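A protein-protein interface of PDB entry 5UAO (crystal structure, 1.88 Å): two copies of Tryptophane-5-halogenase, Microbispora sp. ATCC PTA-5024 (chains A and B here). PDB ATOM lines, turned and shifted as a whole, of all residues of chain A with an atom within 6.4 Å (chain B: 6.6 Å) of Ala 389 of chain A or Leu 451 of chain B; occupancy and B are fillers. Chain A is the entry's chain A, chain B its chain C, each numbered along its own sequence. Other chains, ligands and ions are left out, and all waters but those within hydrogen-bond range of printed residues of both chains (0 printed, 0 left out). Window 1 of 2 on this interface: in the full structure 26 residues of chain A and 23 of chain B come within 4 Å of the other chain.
Among the printed residues, pairs that only touch across the chains: Leu 372 of chain A with Leu 434 of chain B (3.5 Å), Ala 389 of chain A with Leu 451 of chain B (3.7 Å) and Ile 368 of chain A with Phe 447 of chain B (3.7 Å).
Of the printed residues of chain A, Phe 447 of chain B touches Ile 368.
Printed residues of chain B within 4 Å of Leu 372 of chain A: Leu 434.
Printed residues of chain B within 4 Å of Ile 368 of chain A: Phe 447.
Printed residues of chain A within 4 Å of Leu 434 of chain B: Leu 372 (3.5 Å).
Asp 384 of chain A touches none of the printed residues of chain B.
The nearest printed residue of chain B that does not touch Ala 389 of chain A is Phe 447 of chain B (7.2 Å).
The nearest residue of chain A that does not touch Leu 451 of chain B is Ile 368 of chain A (4.1 Å).
Printed residues of chain B that touch a printed residue of chain A: Leu 434, Phe 447 and Leu 451.
Hydrophobic or aromatic side chains of chain B within 4 Å of the printed part of chain A: Leu 434, Phe 447 and Leu 451.
Among the printed residues, 3 pairs touch across the chains.
Among the printed residues, no Asp or Glu carboxylate lies within 4 Å of a Lys or Arg side-chain nitrogen of the other chain.
No position is printed for both chains.
Of the 3 pairs that touch across the chains among the printed residues, none has its exchanged pair printed and touching as well.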
ATOM      1  N   MET A 361       8.091  -0.084  -1.949  1.00  0.00           N
ATOM      2  CA  MET A 361       6.720   0.039  -2.399  1.00  0.00           C
ATOM      3  C   MET A 361       5.671   0.071  -1.294  1.00  0.00           C
ATOM      4  O   MET A 361       4.547   0.623  -1.497  1.00  0.00           O
ATOM      5  CB  MET A 361       6.431  -1.044  -3.427  1.00  0.00           C
ATOM      6  CG  MET A 361       7.130  -0.772  -4.744  1.00  0.00           C
ATOM      7  SD  MET A 361       7.128   0.950  -5.405  1.00  0.00           S
ATOM      8  CE  MET A 361       5.360   1.243  -5.659  1.00  0.00           C
ATOM      9  N   ILE A 368       1.072   7.468   0.182  1.00  0.00           N
ATOM     10  CA  ILE A 368      -0.157   7.713  -0.561  1.00  0.00           C
ATOM     11  C   ILE A 368      -1.384   7.703   0.358  1.00  0.00           C
ATOM     12  O   ILE A 368      -2.192   8.659   0.373  1.00  0.00           O
ATOM     13  CB  ILE A 368      -0.305   6.683  -1.708  1.00  0.00           C
ATOM     14  CG1 ILE A 368       0.751   6.953  -2.794  1.00  0.00           C
ATOM     15  CG2 ILE A 368      -1.680   6.683  -2.349  1.00  0.00           C
ATOM     16  CD1 ILE A 368       0.744   5.902  -3.868  1.00  0.00           C
ATOM     17  N   LEU A 372      -3.572  11.005   1.421  1.00  0.00           N
ATOM     18  CA  LEU A 372      -4.820  11.109   0.721  1.00  0.00           C
ATOM     19  C   LEU A 372      -6.080  10.645   1.484  1.00  0.00           C
ATOM     20  O   LEU A 372      -7.192  10.856   1.003  1.00  0.00           O
ATOM     21  CB  LEU A 372      -4.744  10.383  -0.624  1.00  0.00           C
ATOM     22  CG  LEU A 372      -3.744  10.883  -1.651  1.00  0.00           C
ATOM     23  CD1 LEU A 372      -3.971  10.138  -2.970  1.00  0.00           C
ATOM     24  CD2 LEU A 372      -3.831  12.367  -1.868  1.00  0.00           C
ATOM     25  N   ASP A 384      -8.746   6.756  -7.539  1.00  0.00           N
ATOM     26  CA  ASP A 384      -8.208   6.528  -8.915  1.00  0.00           C
ATOM     27  C   ASP A 384      -6.764   7.064  -9.048  1.00  0.00           C
ATOM     28  O   ASP A 384      -5.883   6.418  -9.680  1.00  0.00           O
ATOM     29  CB  ASP A 384      -9.081   7.180  -9.970  1.00  0.00           C
ATOM     30  CG  ASP A 384     -10.464   6.563 -10.058  1.00  0.00           C
ATOM     31  OD1 ASP A 384     -10.647   5.334  -9.924  1.00  0.00           O
ATOM     32  OD2 ASP A 384     -11.406   7.334 -10.270  1.00  0.00           O
ATOM     33  N   ALA A 385      -6.484   8.211  -8.450  1.00  0.00           N
ATOM     34  CA  ALA A 385      -5.125   8.768  -8.542  1.00  0.00           C
ATOM     35  C   ALA A 385      -4.121   7.829  -7.899  1.00  0.00           C
ATOM     36  O   ALA A 385      -3.019   7.623  -8.439  1.00  0.00           O
ATOM     37  CB  ALA A 385      -5.015  10.104  -7.876  1.00  0.00           C
ATOM     38  N   ALA A 386      -4.491   7.307  -6.727  1.00  0.00           N
ATOM     39  CA  ALA A 386      -3.649   6.379  -5.985  1.00  0.00           C
ATOM     40  C   ALA A 386      -3.445   5.147  -6.811  1.00  0.00           C
ATOM     41  O   ALA A 386      -2.317   4.707  -6.968  1.00  0.00           O
ATOM     42  CB  ALA A 386      -4.274   6.013  -4.634  1.00  0.00           C
ATOM     43  N   ASN A 387      -4.512   4.599  -7.400  1.00  0.00           N
ATOM     44  CA  ASN A 387      -4.371   3.380  -8.177  1.00  0.00           C
ATOM     45  C   ASN A 387      -3.495   3.479  -9.410  1.00  0.00           C
ATOM     46  O   ASN A 387      -2.730   2.524  -9.756  1.00  0.00           O
ATOM     47  CB  ASN A 387      -5.730   2.856  -8.594  1.00  0.00           C
ATOM     48  CG  ASN A 387      -6.556   2.392  -7.386  1.00  0.00           C
ATOM     49  OD1 ASN A 387      -5.987   2.004  -6.374  1.00  0.00           O
ATOM     50  ND2 ASN A 387      -7.861   2.400  -7.508  1.00  0.00           N
ATOM     51  N   GLN A 388      -3.658   4.580 -10.151  1.00  0.00           N
ATOM     52  CA  GLN A 388      -2.821   4.834 -11.308  1.00  0.00           C
ATOM     53  C   GLN A 388      -1.370   5.050 -10.957  1.00  0.00           C
ATOM     54  O   GLN A 388      -0.499   4.620 -11.669  1.00  0.00           O
ATOM     55  CB  GLN A 388      -3.355   6.080 -12.076  1.00  0.00           C
ATOM     56  CG  GLN A 388      -4.647   5.778 -12.793  1.00  0.00           C
ATOM     57  CD  GLN A 388      -5.263   7.022 -13.449  1.00  0.00           C
ATOM     58  OE1 GLN A 388      -4.803   8.151 -13.247  1.00  0.00           O
ATOM     59  NE2 GLN A 388      -6.352   6.812 -14.174  1.00  0.00           N
ATOM     60  N   ALA A 389      -1.085   5.717  -9.852  1.00  0.00           N
ATOM     61  CA  ALA A 389       0.286   5.988  -9.475  1.00  0.00           C
ATOM     62  C   ALA A 389       0.966   4.686  -9.092  1.00  0.00           C
ATOM     63  O   ALA A 389       2.127   4.401  -9.518  1.00  0.00           O
ATOM     64  CB  ALA A 389       0.363   6.970  -8.310  1.00  0.00           C
ATOM     65  N   LEU A 390       0.259   3.882  -8.314  1.00  0.00           N
ATOM     66  CA  LEU A 390       0.834   2.585  -7.915  1.00  0.00           C
ATOM     67  C   LEU A 390       1.009   1.603  -9.067  1.00  0.00           C
ATOM     68  O   LEU A 390       2.043   0.911  -9.157  1.00  0.00           O
ATOM     69  CB  LEU A 390       0.021   1.955  -6.763  1.00  0.00           C
ATOM     70  CG  LEU A 390       0.342   2.614  -5.404  1.00  0.00           C
ATOM     71  CD1 LEU A 390      -0.747   2.329  -4.376  1.00  0.00           C
ATOM     72  CD2 LEU A 390       1.717   2.223  -4.913  1.00  0.00           C
ATOM     73  N   ALA A 391       0.024   1.503  -9.924  1.00  0.00           N
ATOM     74  CA  ALA A 391       0.152   0.630 -11.089  1.00  0.00           C
ATOM     75  C   ALA A 391       1.394   1.046 -11.918  1.00  0.00           C
ATOM     76  O   ALA A 391       2.103   0.201 -12.449  1.00  0.00           O
ATOM     77  CB  ALA A 391      -1.093   0.720 -11.996  1.00  0.00           C
ATOM     78  N   HIS A 392       1.593   2.339 -12.107  1.00  0.00           N
ATOM     79  CA  HIS A 392       2.664   2.790 -13.018  1.00  0.00           C
ATOM     80  C   HIS A 392       4.062   2.446 -12.399  1.00  0.00           C
ATOM     81  O   HIS A 392       4.995   2.000 -13.067  1.00  0.00           O
ATOM     82  CB  HIS A 392       2.528   4.319 -13.214  1.00  0.00           C
ATOM     83  CG  HIS A 392       3.652   4.926 -13.982  1.00  0.00           C
ATOM     84  ND1 HIS A 392       3.824   4.706 -15.329  1.00  0.00           N
ATOM     85  CD2 HIS A 392       4.699   5.686 -13.592  1.00  0.00           C
ATOM     86  CE1 HIS A 392       4.897   5.351 -15.751  1.00  0.00           C
ATOM     87  NE2 HIS A 392       5.439   5.963 -14.718  1.00  0.00           N
ATOM     88  N   ARG A 393       4.177   2.682 -11.107  1.00  0.00           N
ATOM     89  CA  ARG A 393       5.414   2.414 -10.372  1.00  0.00           C
ATOM     90  C   ARG A 393       5.718   0.910 -10.386  1.00  0.00           C
ATOM     91  O   ARG A 393       6.831   0.522 -10.709  1.00  0.00           O
ATOM     92  CB  ARG A 393       5.319   2.946  -8.924  1.00  0.00           C
ATOM     93  CG  ARG A 393       5.771   4.417  -8.834  1.00  0.00           C
ATOM     94  CD  ARG A 393       7.337   4.509  -8.629  1.00  0.00           C
ATOM     95  NE  ARG A 393       7.488   5.136  -7.323  1.00  0.00           N
ATOM     96  CZ  ARG A 393       8.368   4.910  -6.399  1.00  0.00           C
ATOM     97  NH1 ARG A 393       9.393   4.099  -6.555  1.00  0.00           N
ATOM     98  NH2 ARG A 393       8.214   5.589  -5.276  1.00  0.00           N
ATOM     99  N   TRP A 394       4.723   0.051 -10.093  1.00  0.00           N
ATOM    100  CA  TRP A 394       4.959  -1.381 -10.084  1.00  0.00           C
ATOM    101  C   TRP A 394       5.291  -1.930 -11.487  1.00  0.00           C
ATOM    102  O   TRP A 394       6.202  -2.744 -11.678  1.00  0.00           O
ATOM    103  CB  TRP A 394       3.769  -2.084  -9.451  1.00  0.00           C
ATOM    104  CG  TRP A 394       3.777  -2.124  -7.963  1.00  0.00           C
ATOM    105  CD1 TRP A 394       3.177  -1.251  -7.112  1.00  0.00           C
ATOM    106  CD2 TRP A 394       4.419  -3.110  -7.146  1.00  0.00           C
ATOM    107  NE1 TRP A 394       3.357  -1.655  -5.813  1.00  0.00           N
ATOM    108  CE2 TRP A 394       4.138  -2.779  -5.798  1.00  0.00           C
ATOM    109  CE3 TRP A 394       5.239  -4.209  -7.411  1.00  0.00           C
ATOM    110  CZ2 TRP A 394       4.608  -3.540  -4.720  1.00  0.00           C
ATOM    111  CZ3 TRP A 394       5.704  -4.987  -6.316  1.00  0.00           C
ATOM    112  CH2 TRP A 394       5.413  -4.611  -4.996  1.00  0.00           C
ATOM    113  N   LEU B 431      -7.275  13.498 -11.293  1.00  0.00           N
ATOM    114  CA  LEU B 431      -6.734  14.761 -10.787  1.00  0.00           C
ATOM    115  C   LEU B 431      -7.799  15.763 -10.280  1.00  0.00           C
ATOM    116  O   LEU B 431      -7.569  16.530  -9.331  1.00  0.00           O
ATOM    117  CB  LEU B 431      -5.904  15.409 -11.921  1.00  0.00           C
ATOM    118  CG  LEU B 431      -5.184  16.678 -11.671  1.00  0.00           C
ATOM    119  CD1 LEU B 431      -4.137  16.336 -10.634  1.00  0.00           C
ATOM    120  CD2 LEU B 431      -4.475  17.167 -12.930  1.00  0.00           C
ATOM    121  N   LEU B 434      -8.743  14.881  -6.810  1.00  0.00           N
ATOM    122  CA  LEU B 434      -7.676  15.391  -5.957  1.00  0.00           C
ATOM    123  C   LEU B 434      -7.776  16.890  -5.694  1.00  0.00           C
ATOM    124  O   LEU B 434      -7.541  17.365  -4.565  1.00  0.00           O
ATOM    125  CB  LEU B 434      -6.313  15.034  -6.574  1.00  0.00           C
ATOM    126  CG  LEU B 434      -5.028  14.770  -5.800  1.00  0.00           C
ATOM    127  CD1 LEU B 434      -5.274  13.773  -4.677  1.00  0.00           C
ATOM    128  CD2 LEU B 434      -3.932  14.259  -6.752  1.00  0.00           C
ATOM    129  N   SER B 446       4.208  18.397  -0.569  1.00  0.00           N
ATOM    130  CA  SER B 446       5.109  18.067  -1.679  1.00  0.00           C
ATOM    131  C   SER B 446       4.856  16.747  -2.302  1.00  0.00           C
ATOM    132  O   SER B 446       5.079  16.580  -3.511  1.00  0.00           O
ATOM    133  CB  SER B 446       6.583  18.115  -1.244  1.00  0.00           C
ATOM    134  OG  SER B 446       6.813  19.213  -0.384  1.00  0.00           O
ATOM    135  N   PHE B 447       4.440  15.773  -1.485  1.00  0.00           N
ATOM    136  CA  PHE B 447       4.291  14.435  -2.014  1.00  0.00           C
ATOM    137  C   PHE B 447       3.047  14.358  -2.912  1.00  0.00           C
ATOM    138  O   PHE B 447       3.081  13.777  -4.014  1.00  0.00           O
ATOM    139  CB  PHE B 447       4.275  13.358  -0.883  1.00  0.00           C
ATOM    140  CG  PHE B 447       4.104  11.948  -1.387  1.00  0.00           C
ATOM    141  CD1 PHE B 447       5.187  11.216  -1.841  1.00  0.00           C
ATOM    142  CD2 PHE B 447       2.845  11.370  -1.467  1.00  0.00           C
ATOM    143  CE1 PHE B 447       5.021   9.924  -2.340  1.00  0.00           C
ATOM    144  CE2 PHE B 447       2.673  10.084  -1.942  1.00  0.00           C
ATOM    145  CZ  PHE B 447       3.765   9.353  -2.381  1.00  0.00           C
ATOM    146  N   THR B 448       1.960  14.932  -2.434  1.00  0.00           N
ATOM    147  CA  THR B 448       0.703  14.973  -3.175  1.00  0.00           C
ATOM    148  C   THR B 448       0.950  15.776  -4.457  1.00  0.00           C
ATOM    149  O   THR B 448       0.573  15.342  -5.571  1.00  0.00           O
ATOM    150  CB  THR B 448      -0.393  15.624  -2.321  1.00  0.00           C
ATOM    151  OG1 THR B 448      -0.666  14.818  -1.165  1.00  0.00           O
ATOM    152  CG2 THR B 448      -1.640  15.816  -3.098  1.00  0.00           C
ATOM    153  N   ARG B 449       1.630  16.912  -4.330  1.00  0.00           N
ATOM    154  CA  ARG B 449       1.928  17.734  -5.541  1.00  0.00           C
ATOM    155  C   ARG B 449       2.679  16.942  -6.568  1.00  0.00           C
ATOM    156  O   ARG B 449       2.358  16.918  -7.782  1.00  0.00           O
ATOM    157  CB  ARG B 449       2.790  18.937  -5.214  1.00  0.00           C
ATOM    158  CG  ARG B 449       2.036  20.160  -4.806  1.00  0.00           C
ATOM    159  CD  ARG B 449       2.965  21.363  -4.737  1.00  0.00           C
ATOM    160  NE  ARG B 449       3.753  21.380  -3.491  1.00  0.00           N
ATOM    161  CZ  ARG B 449       5.080  21.432  -3.439  1.00  0.00           C
ATOM    162  NH1 ARG B 449       5.805  21.485  -4.555  1.00  0.00           N
ATOM    163  NH2 ARG B 449       5.698  21.445  -2.264  1.00  0.00           N
ATOM    164  N   TYR B 450       3.685  16.235  -6.082  1.00  0.00           N
ATOM    165  CA  TYR B 450       4.475  15.417  -6.952  1.00  0.00           C
ATOM    166  C   TYR B 450       3.642  14.341  -7.658  1.00  0.00           C
ATOM    167  O   TYR B 450       3.806  14.030  -8.844  1.00  0.00           O
ATOM    168  CB  TYR B 450       5.660  14.834  -6.143  1.00  0.00           C
ATOM    169  CG  TYR B 450       6.582  14.088  -7.055  1.00  0.00           C
ATOM    170  CD1 TYR B 450       7.532  14.763  -7.836  1.00  0.00           C
ATOM    171  CD2 TYR B 450       6.436  12.709  -7.231  1.00  0.00           C
ATOM    172  CE1 TYR B 450       8.349  14.071  -8.728  1.00  0.00           C
ATOM    173  CE2 TYR B 450       7.242  12.009  -8.120  1.00  0.00           C
ATOM    174  CZ  TYR B 450       8.197  12.692  -8.859  1.00  0.00           C
ATOM    175  OH  TYR B 450       8.986  11.969  -9.711  1.00  0.00           O
ATOM    176  N   LEU B 451       2.737  13.738  -6.916  1.00  0.00           N
ATOM    177  CA  LEU B 451       1.854  12.710  -7.481  1.00  0.00           C
ATOM    178  C   LEU B 451       0.843  13.327  -8.515  1.00  0.00           C
ATOM    179  O   LEU B 451       0.564  12.802  -9.564  1.00  0.00           O
ATOM    180  CB  LEU B 451       1.115  12.032  -6.320  1.00  0.00           C
ATOM    181  CG  LEU B 451       0.359  10.805  -6.794  1.00  0.00           C
ATOM    182  CD1 LEU B 451       0.517   9.647  -5.818  1.00  0.00           C
ATOM    183  CD2 LEU B 451      -1.069  11.235  -6.938  1.00  0.00           C
ATOM    184  N   ALA B 452       0.274  14.446  -8.171  1.00  0.00           N
ATOM    185  CA  ALA B 452      -0.681  15.098  -9.052  1.00  0.00           C
ATOM    186  C   ALA B 452       0.001  15.549 -10.358  1.00  0.00           C
ATOM    187  O   ALA B 452      -0.630  15.536 -11.416  1.00  0.00           O
ATOM    188  CB  ALA B 452      -1.270  16.297  -8.344  1.00  0.00           C
ATOM    189  N   ASP B 453       1.279  15.915 -10.250  1.00  0.00           N
ATOM    190  CA  ASP B 453       2.073  16.376 -11.386  1.00  0.00           C
ATOM    191  C   ASP B 453       2.015  15.503 -12.598  1.00  0.00           C
ATOM    192  O   ASP B 453       1.983  16.030 -13.677  1.00  0.00           O
ATOM    193  CB  ASP B 453       3.515  16.638 -11.021  1.00  0.00           C
ATOM    194  CG  ASP B 453       4.050  17.889 -11.686  1.00  0.00           C
ATOM    195  OD1 ASP B 453       3.498  18.294 -12.726  1.00  0.00           O
ATOM    196  OD2 ASP B 453       5.012  18.483 -11.156  1.00  0.00           O
ATOM    197  N   GLY B 454       1.902  14.189 -12.445  1.00  0.00           N
ATOM    198  CA  GLY B 454       1.924  13.296 -13.598  1.00  0.00           C
ATOM    199  C   GLY B 454       0.684  13.317 -14.437  1.00  0.00           C
ATOM    200  O   GLY B 454       0.716  12.875 -15.616  1.00  0.00           O
ATOM    201  N   ALA B 455      -0.425  13.834 -13.882  1.00  0.00           N
ATOM    202  CA  ALA B 455      -1.654  13.958 -14.705  1.00  0.00           C
ATOM    203  C   ALA B 455      -1.735  15.270 -15.495  1.00  0.00           C
ATOM    204  O   ALA B 455      -2.507  15.413 -16.475  1.00  0.00           O
ATOM    205  CB  ALA B 455      -2.888  13.737 -13.844  1.00  0.00           C
ATOM    206  N   LEU B 462       0.689  21.759 -13.183  1.00  0.00           N
ATOM    207  CA  LEU B 462      -0.349  21.888 -12.184  1.00  0.00           C
ATOM    208  C   LEU B 462      -0.867  23.325 -12.041  1.00  0.00           C
ATOM    209  O   LEU B 462      -2.026  23.543 -11.732  1.00  0.00           O
ATOM    210  CB  LEU B 462       0.164  21.499 -10.835  1.00  0.00           C
ATOM    211  CG  LEU B 462       0.268  20.019 -10.507  1.00  0.00           C
ATOM    212  CD1 LEU B 462       0.750  19.974  -9.051  1.00  0.00           C
ATOM    213  CD2 LEU B 462      -1.007  19.210 -10.672  1.00  0.00           C
